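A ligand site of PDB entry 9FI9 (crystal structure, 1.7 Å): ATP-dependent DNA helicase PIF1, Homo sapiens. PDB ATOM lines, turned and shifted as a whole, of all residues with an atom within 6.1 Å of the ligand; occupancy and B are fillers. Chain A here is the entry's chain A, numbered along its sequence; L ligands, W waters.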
ATOM      1  N   GLY A  55       7.961  -9.777  32.795  1.00  0.00           N
ATOM      2  CA  GLY A  55       7.458 -10.804  31.885  1.00  0.00           C
ATOM      3  C   GLY A  55       8.513 -11.344  30.918  1.00  0.00           C
ATOM      4  O   GLY A  55       8.683 -12.548  30.787  1.00  0.00           O
ATOM      5  N   VAL A  56       9.255 -10.447  30.243  1.00  0.00           N
ATOM      6  CA  VAL A  56      10.270 -10.891  29.304  1.00  0.00           C
ATOM      7  C   VAL A  56      11.294 -11.786  29.998  1.00  0.00           C
ATOM      8  O   VAL A  56      11.634 -12.855  29.501  1.00  0.00           O
ATOM      9  CB  VAL A  56      10.961  -9.746  28.542  1.00  0.00           C
ATOM     10  CG1 VAL A  56       9.945  -8.922  27.760  1.00  0.00           C
ATOM     11  CG2 VAL A  56      11.772  -8.849  29.471  1.00  0.00           C
ATOM     12  N   ALA A  57      11.756 -11.372  31.180  1.00  0.00           N
ATOM     13  CA  ALA A  57      12.774 -12.155  31.884  1.00  0.00           C
ATOM     14  C   ALA A  57      12.192 -13.477  32.398  1.00  0.00           C
ATOM     15  O   ALA A  57      12.904 -14.475  32.505  1.00  0.00           O
ATOM     16  CB  ALA A  57      13.366 -11.338  33.000  1.00  0.00           C
ATOM     17  N   CYS A  59      10.026 -15.386  31.015  1.00  0.00           N
ATOM     18  CA  CYS A  59       9.991 -16.332  29.915  1.00  0.00           C
ATOM     19  C   CYS A  59      11.296 -17.098  29.777  1.00  0.00           C
ATOM     20  O   CYS A  59      11.280 -18.287  29.486  1.00  0.00           O
ATOM     21  CB  CYS A  59       9.811 -15.613  28.585  1.00  0.00           C
ATOM     22  SG  CYS A  59       8.132 -14.983  28.438  1.00  0.00           S
ATOM     23  N   THR A 221      18.284  -4.942  13.564  1.00  0.00           N
ATOM     24  CA  THR A 221      17.219  -4.495  14.451  1.00  0.00           C
ATOM     25  C   THR A 221      17.717  -3.238  15.184  1.00  0.00           C
ATOM     26  O   THR A 221      18.719  -3.313  15.897  1.00  0.00           O
ATOM     27  CB  THR A 221      16.833  -5.578  15.450  1.00  0.00           C
ATOM     28  OG1 THR A 221      16.381  -6.745  14.741  1.00  0.00           O
ATOM     29  CG2 THR A 221      15.733  -5.081  16.402  1.00  0.00           C
ATOM     30  N   GLN A 227       8.729   1.811  23.554  1.00  0.00           N
ATOM     31  CA  GLN A 227       7.902   0.986  22.683  1.00  0.00           C
ATOM     32  C   GLN A 227       7.121   1.826  21.666  1.00  0.00           C
ATOM     33  O   GLN A 227       6.791   1.316  20.585  1.00  0.00           O
ATOM     34  CB  GLN A 227       6.971   0.111  23.539  1.00  0.00           C
ATOM     35  CG  GLN A 227       6.114  -0.880  22.755  1.00  0.00           C
ATOM     36  CD  GLN A 227       6.905  -1.892  21.931  1.00  0.00           C
ATOM     37  OE1 GLN A 227       8.007  -2.301  22.304  1.00  0.00           O
ATOM     38  NE2 GLN A 227       6.376  -2.292  20.776  1.00  0.00           N
ATOM     39  N   VAL A 230       9.304   1.892  18.712  1.00  0.00           N
ATOM     40  CA  VAL A 230       9.382   0.582  18.101  1.00  0.00           C
ATOM     41  C   VAL A 230       8.158   0.319  17.228  1.00  0.00           C
ATOM     42  O   VAL A 230       8.294  -0.095  16.071  1.00  0.00           O
ATOM     43  CB  VAL A 230       9.482  -0.462  19.221  1.00  0.00           C
ATOM     44  CG1 VAL A 230       9.452  -1.879  18.639  1.00  0.00           C
ATOM     45  CG2 VAL A 230      10.740  -0.193  20.065  1.00  0.00           C
ATOM     46  N   ASN A 234       8.236  -0.350  13.142  1.00  0.00           N
ATOM     47  CA  ASN A 234       7.832  -1.623  12.551  1.00  0.00           C
ATOM     48  C   ASN A 234       6.620  -1.455  11.631  1.00  0.00           C
ATOM     49  O   ASN A 234       6.537  -2.129  10.616  1.00  0.00           O
ATOM     50  CB  ASN A 234       7.569  -2.669  13.625  1.00  0.00           C
ATOM     51  CG  ASN A 234       8.846  -3.183  14.256  1.00  0.00           C
ATOM     52  OD1 ASN A 234       9.872  -3.324  13.574  1.00  0.00           O
ATOM     53  ND2 ASN A 234       8.810  -3.473  15.554  1.00  0.00           N
ATOM     54  N   ASP A 262      -0.503 -10.669  27.412  1.00  0.00           N
ATOM     55  CA  ASP A 262       0.457  -9.861  26.676  1.00  0.00           C
ATOM     56  C   ASP A 262       1.670  -9.517  27.539  1.00  0.00           C
ATOM     57  O   ASP A 262       2.795  -9.428  27.028  1.00  0.00           O
ATOM     58  CB  ASP A 262      -0.158  -8.596  26.073  1.00  0.00           C
ATOM     59  CG  ASP A 262      -1.207  -8.815  24.991  1.00  0.00           C
ATOM     60  OD1 ASP A 262      -1.062  -9.794  24.237  1.00  0.00           O
ATOM     61  OD2 ASP A 262      -2.147  -8.004  24.912  1.00  0.00           O
ATOM     62  N   ALA A 263       1.472  -9.360  28.850  1.00  0.00           N
ATOM     63  CA  ALA A 263       2.594  -8.963  29.696  1.00  0.00           C
ATOM     64  C   ALA A 263       3.621 -10.085  29.844  1.00  0.00           C
ATOM     65  O   ALA A 263       4.776  -9.817  30.195  1.00  0.00           O
ATOM     66  CB  ALA A 263       2.109  -8.436  31.025  1.00  0.00           C
ATOM     67  N   GLN A 264       3.256 -11.341  29.553  1.00  0.00           N
ATOM     68  CA  GLN A 264       4.150 -12.433  29.882  1.00  0.00           C
ATOM     69  C   GLN A 264       4.431 -13.328  28.673  1.00  0.00           C
ATOM     70  O   GLN A 264       4.984 -14.425  28.824  1.00  0.00           O
ATOM     71  CB  GLN A 264       3.462 -13.267  30.959  1.00  0.00           C
ATOM     72  CG  GLN A 264       3.560 -12.676  32.361  1.00  0.00           C
ATOM     73  CD  GLN A 264       3.532 -13.779  33.396  1.00  0.00           C
ATOM     74  OE1 GLN A 264       4.427 -14.635  33.443  1.00  0.00           O
ATOM     75  NE2 GLN A 264       2.462 -13.806  34.181  1.00  0.00           N
ATOM     76  N   CYS A 265       4.084 -12.821  27.488  1.00  0.00           N
ATOM     77  CA  CYS A 265       4.136 -13.597  26.251  1.00  0.00           C
ATOM     78  C   CYS A 265       4.726 -12.716  25.135  1.00  0.00           C
ATOM     79  O   CYS A 265       4.350 -11.561  25.029  1.00  0.00           O
ATOM     80  CB  CYS A 265       2.723 -14.089  25.980  1.00  0.00           C
ATOM     81  SG  CYS A 265       2.423 -14.582  24.267  1.00  0.00           S
ATOM     82  N   PRO A 266       5.708 -13.194  24.301  1.00  0.00           N
ATOM     83  CA  PRO A 266       6.331 -12.352  23.276  1.00  0.00           C
ATOM     84  C   PRO A 266       5.614 -12.190  21.929  1.00  0.00           C
ATOM     85  O   PRO A 266       6.134 -11.512  21.034  1.00  0.00           O
ATOM     86  CB  PRO A 266       7.680 -13.069  23.111  1.00  0.00           C
ATOM     87  CG  PRO A 266       7.332 -14.538  23.223  1.00  0.00           C
ATOM     88  CD  PRO A 266       6.273 -14.550  24.326  1.00  0.00           C
ATOM     89  N   VAL A 267       4.437 -12.814  21.781  1.00  0.00           N
ATOM     90  CA  VAL A 267       3.740 -12.703  20.496  1.00  0.00           C
ATOM     91  C   VAL A 267       2.417 -11.973  20.689  1.00  0.00           C
ATOM     92  O   VAL A 267       1.843 -11.992  21.776  1.00  0.00           O
ATOM     93  CB  VAL A 267       3.543 -14.091  19.846  1.00  0.00           C
ATOM     94  CG1 VAL A 267       4.844 -14.621  19.252  1.00  0.00           C
ATOM     95  CG2 VAL A 267       2.923 -15.067  20.835  1.00  0.00           C
ATOM     96  N   MET A 280      11.797 -11.513  13.956  1.00  0.00           N
ATOM     97  CA  MET A 280      12.622 -12.135  14.964  1.00  0.00           C
ATOM     98  C   MET A 280      11.888 -13.378  15.454  1.00  0.00           C
ATOM     99  O   MET A 280      10.696 -13.314  15.734  1.00  0.00           O
ATOM    100  CB  MET A 280      12.876 -11.178  16.125  1.00  0.00           C
ATOM    101  CG  MET A 280      13.679 -11.855  17.212  1.00  0.00           C
ATOM    102  SD  MET A 280      14.117 -10.668  18.515  1.00  0.00           S
ATOM    103  CE  MET A 280      15.180  -9.470  17.703  1.00  0.00           C
ATOM    104  N   VAL A 282      11.025 -15.786  18.388  1.00  0.00           N
ATOM    105  CA  VAL A 282      10.906 -15.403  19.790  1.00  0.00           C
ATOM    106  C   VAL A 282      10.638 -16.629  20.661  1.00  0.00           C
ATOM    107  O   VAL A 282      10.110 -16.505  21.774  1.00  0.00           O
ATOM    108  CB  VAL A 282       9.883 -14.275  20.029  1.00  0.00           C
ATOM    109  CG1 VAL A 282      10.414 -12.940  19.490  1.00  0.00           C
ATOM    110  CG2 VAL A 282       8.516 -14.598  19.436  1.00  0.00           C
ATOM    111  N   GLN A 345       7.937 -11.898  15.733  1.00  0.00           N
ATOM    112  CA  GLN A 345       7.614 -10.487  15.899  1.00  0.00           C
ATOM    113  C   GLN A 345       8.316  -9.708  14.786  1.00  0.00           C
ATOM    114  O   GLN A 345       9.375 -10.134  14.321  1.00  0.00           O
ATOM    115  CB  GLN A 345       8.220  -9.972  17.216  1.00  0.00           C
ATOM    116  CG  GLN A 345       7.423 -10.333  18.473  1.00  0.00           C
ATOM    117  CD  GLN A 345       6.204  -9.466  18.722  1.00  0.00           C
ATOM    118  OE1 GLN A 345       5.959  -8.473  18.021  1.00  0.00           O
ATOM    119  NE2 GLN A 345       5.443  -9.818  19.747  1.00  0.00           N
ATOM    120  N   LEU A 346       7.744  -8.565  14.377  1.00  0.00           N
ATOM    121  CA  LEU A 346       8.431  -7.675  13.447  1.00  0.00           C
ATOM    122  C   LEU A 346       9.647  -7.111  14.167  1.00  0.00           C
ATOM    123  O   LEU A 346       9.587  -6.910  15.385  1.00  0.00           O
ATOM    124  CB  LEU A 346       7.484  -6.551  13.022  1.00  0.00           C
ATOM    125  CG  LEU A 346       6.232  -6.996  12.248  1.00  0.00           C
ATOM    126  CD1 LEU A 346       5.462  -5.749  11.898  1.00  0.00           C
ATOM    127  CD2 LEU A 346       6.647  -7.762  11.049  1.00  0.00           C
ATOM    128  N   ALA A 347      10.750  -6.887  13.427  1.00  0.00           N
ATOM    129  CA  ALA A 347      12.023  -6.665  14.101  1.00  0.00           C
ATOM    130  C   ALA A 347      12.903  -5.671  13.335  1.00  0.00           C
ATOM    131  O   ALA A 347      14.130  -5.750  13.427  1.00  0.00           O
ATOM    132  CB  ALA A 347      12.758  -7.973  14.333  1.00  0.00           C
ATOM    133  N   ALA A 349      12.721  -2.902  14.535  1.00  0.00           N
ATOM    134  CA  ALA A 349      13.002  -2.234  15.831  1.00  0.00           C
ATOM    135  C   ALA A 349      12.526  -3.115  16.977  1.00  0.00           C
ATOM    136  O   ALA A 349      11.625  -3.952  16.783  1.00  0.00           O
ATOM    137  CB  ALA A 349      12.289  -0.892  15.921  1.00  0.00           C
ATOM    138  N   MET A 350      13.084  -2.842  18.164  1.00  0.00           N
ATOM    139  CA  MET A 350      12.852  -3.569  19.385  1.00  0.00           C
ATOM    140  C   MET A 350      13.190  -2.655  20.561  1.00  0.00           C
ATOM    141  O   MET A 350      14.135  -1.878  20.470  1.00  0.00           O
ATOM    142  CB  MET A 350      13.830  -4.746  19.426  1.00  0.00           C
ATOM    143  CG  MET A 350      13.646  -5.635  20.600  1.00  0.00           C
ATOM    144  SD  MET A 350      14.780  -7.034  20.490  1.00  0.00           S
ATOM    145  CE  MET A 350      14.084  -8.164  21.714  1.00  0.00           C
ATOM    146  N   SER A 351      12.430  -2.733  21.667  1.00  0.00           N
ATOM    147  CA  SER A 351      12.792  -1.900  22.819  1.00  0.00           C
ATOM    148  C   SER A 351      13.940  -2.527  23.601  1.00  0.00           C
ATOM    149  O   SER A 351      14.073  -3.736  23.644  1.00  0.00           O
ATOM    150  CB  SER A 351      11.615  -1.580  23.742  1.00  0.00           C
ATOM    151  OG  SER A 351      11.439  -2.634  24.667  1.00  0.00           O
ATOM    152  N   LYS A 354      12.618  -5.006  26.087  1.00  0.00           N
ATOM    153  CA  LYS A 354      12.263  -6.332  25.599  1.00  0.00           C
ATOM    154  C   LYS A 354      13.471  -7.220  25.294  1.00  0.00           C
ATOM    155  O   LYS A 354      13.313  -8.426  25.130  1.00  0.00           O
ATOM    156  CB  LYS A 354      11.372  -6.267  24.349  1.00  0.00           C
ATOM    157  CG  LYS A 354      10.018  -5.634  24.635  1.00  0.00           C
ATOM    158  CD  LYS A 354       9.310  -6.252  25.818  1.00  0.00           C
ATOM    159  CE  LYS A 354       7.903  -5.761  25.921  1.00  0.00           C
ATOM    160  NZ  LYS A 354       7.226  -6.508  26.992  1.00  0.00           N
ATOM    161  N   SER A 355      14.661  -6.634  25.173  1.00  0.00           N
ATOM    162  CA  SER A 355      15.895  -7.393  24.894  1.00  0.00           C
ATOM    163  C   SER A 355      16.527  -7.907  26.188  1.00  0.00           C
ATOM    164  O   SER A 355      17.519  -8.619  26.128  1.00  0.00           O
ATOM    165  CB  SER A 355      16.925  -6.576  24.176  1.00  0.00           C
ATOM    166  OG  SER A 355      17.538  -5.636  25.059  1.00  0.00           O
ATOM    167  N   MET A 358      18.423 -11.321  26.774  1.00  0.00           N
ATOM    168  CA  MET A 358      18.535 -12.002  25.485  1.00  0.00           C
ATOM    169  C   MET A 358      19.923 -11.908  24.879  1.00  0.00           C
ATOM    170  O   MET A 358      20.701 -11.003  25.205  1.00  0.00           O
ATOM    171  CB  MET A 358      17.610 -11.380  24.429  1.00  0.00           C
ATOM    172  CG  MET A 358      16.138 -11.648  24.756  1.00  0.00           C
ATOM    173  SD  MET A 358      15.054 -11.106  23.419  1.00  0.00           S
ATOM    174  CE  MET A 358      15.459 -12.261  22.096  1.00  0.00           C
HETATM  175  N1  LIG L   1       9.731  -5.657  18.237  1.00  0.00           N
HETATM  176  C1  LIG L   1      10.390  -9.692  22.691  1.00  0.00           C
HETATM  177  C2  LIG L   1       9.576  -8.878  21.884  1.00  0.00           C
HETATM  178  C3  LIG L   1       8.266  -8.617  22.311  1.00  0.00           C
HETATM  179  C4  LIG L   1       7.802  -9.131  23.508  1.00  0.00           C
HETATM  180  C5  LIG L   1      10.078  -8.324  20.604  1.00  0.00           C
HETATM  181  C6  LIG L   1      10.093  -6.789  18.990  1.00  0.00           C
HETATM  182  N2  LIG L   1       8.163 -10.493  25.532  1.00  0.00           N
HETATM  183  C7  LIG L   1       6.922 -10.931  27.581  1.00  0.00           C
HETATM  184  O1  LIG L   1       6.433  -9.128  26.081  1.00  0.00           O
HETATM  185  C8  LIG L   1       7.130 -10.119  26.325  1.00  0.00           C
HETATM  186  C9  LIG L   1       8.615  -9.937  24.308  1.00  0.00           C
HETATM  187  C10 LIG L   1       9.917 -10.195  23.887  1.00  0.00           C
HETATM  188  C11 LIG L   1      11.001  -8.899  19.787  1.00  0.00           C
HETATM  189  N3  LIG L   1       9.564  -7.124  20.145  1.00  0.00           N
HETATM  190  S1  LIG L   1      11.279  -7.895  18.375  1.00  0.00           S
HETATM  191  O   HOH W   1      10.106  -4.224  21.497  1.00  0.00           O
HETATM  192  O   HOH W   2       6.928  -5.100  19.364  1.00  0.00           O
HETATM  193  O   HOH W   3       7.068  -6.300  16.727  1.00  0.00           O
HETATM  194  O   HOH W   4       5.884  -7.519  29.038  1.00  0.00           O
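O of Leu 346 is in hydrogen-bond range of N1 of the ligand (3.1 Å). O of Ala 349 is in hydrogen-bond range of N1 of the ligand, at 2.9 Å. The side-chain amino group (NZ) of Lys 354 is in hydrogen-bond range of an oxygen (O1) of the ligand (2.9 Å).
The side-chain hydroxyl (OG) of Ser 351 lies within hydrogen-bond range of the backbone NH (N) of Lys 354. The backbone carbonyl oxygen of Val 230 sits at hydrogen-bond distance from the side-chain amide nitrogen of Asn 234, 3.5 Å away. The side-chain sulfur (SG) of Cys 59 sits at hydrogen-bond distance from the backbone carbonyl oxygen (O) of Gln 264 (3.2 Å). The backbone NH (N) of Ala 349 sits at hydrogen-bond distance from the side-chain amide oxygen (OD1) of Asn 234 (3.0 Å). The side-chain sulfur (SG) of Cys 265 sits close to the backbone carbonyl oxygen (O) of Val 267 (3.6 Å). N of Met 280 sits at hydrogen-bond distance from O of Gln 345, at 2.8 Å. O of Gly 55 is in hydrogen-bond range of SG of Cys 59.
O of Cys 265 sits close to O1 of the ligand (3.4 Å). C of Gly 55 touches C7 of the ligand, at 3.7 Å. Val 56 touches the ligand. Val 230 touches the ligand (CG1 to N1, 3.8 Å). Asn 234 touches the ligand. Asp 262 touches the ligand. Ala 263 touches the ligand. C of Gln 264 touches C7 of the ligand (3.6 Å). Pro 266 touches the ligand (CA to N2, 3.4 Å). Met 280 touches the ligand (SD to C11, 3.8 Å). CB of Gln 345 touches S1 of the ligand (3.9 Å). CE of Met 350 touches C11 of the ligand, at 3.7 Å. Hydrophobic or aromatic side chains that line the ligand: Val 56, Val 230, Pro 266, Met 280 and Met 350. 15 residues have an atom within 4 Å of the ligand: Gly 55, Val 56, Val 230, Asn 234, Asp 262, Ala 263, Gln 264, Cys 265, Pro 266, Met 280, Gln 345, Leu 346, Ala 349, Met 350 and Lys 354.
Water W2 bridges N1 of the ligand (3.1 Å) and NE2 of Gln 227 (3.2 Å). Water W3 lies within hydrogen-bond range of OE1 of Gln 345 (2.8 Å), O of Leu 346 (2.9 Å) and N1 of the ligand (3.1 Å). Water W1 lies within hydrogen-bond range of N of Ser 351, OE1 of Gln 227 and N3 of the ligand. Water W4 lies within hydrogen-bond range of NZ of Lys 354 (2.6 Å), O of Ala 263 (2.8 Å) and O1 of the ligand (3.4 Å).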
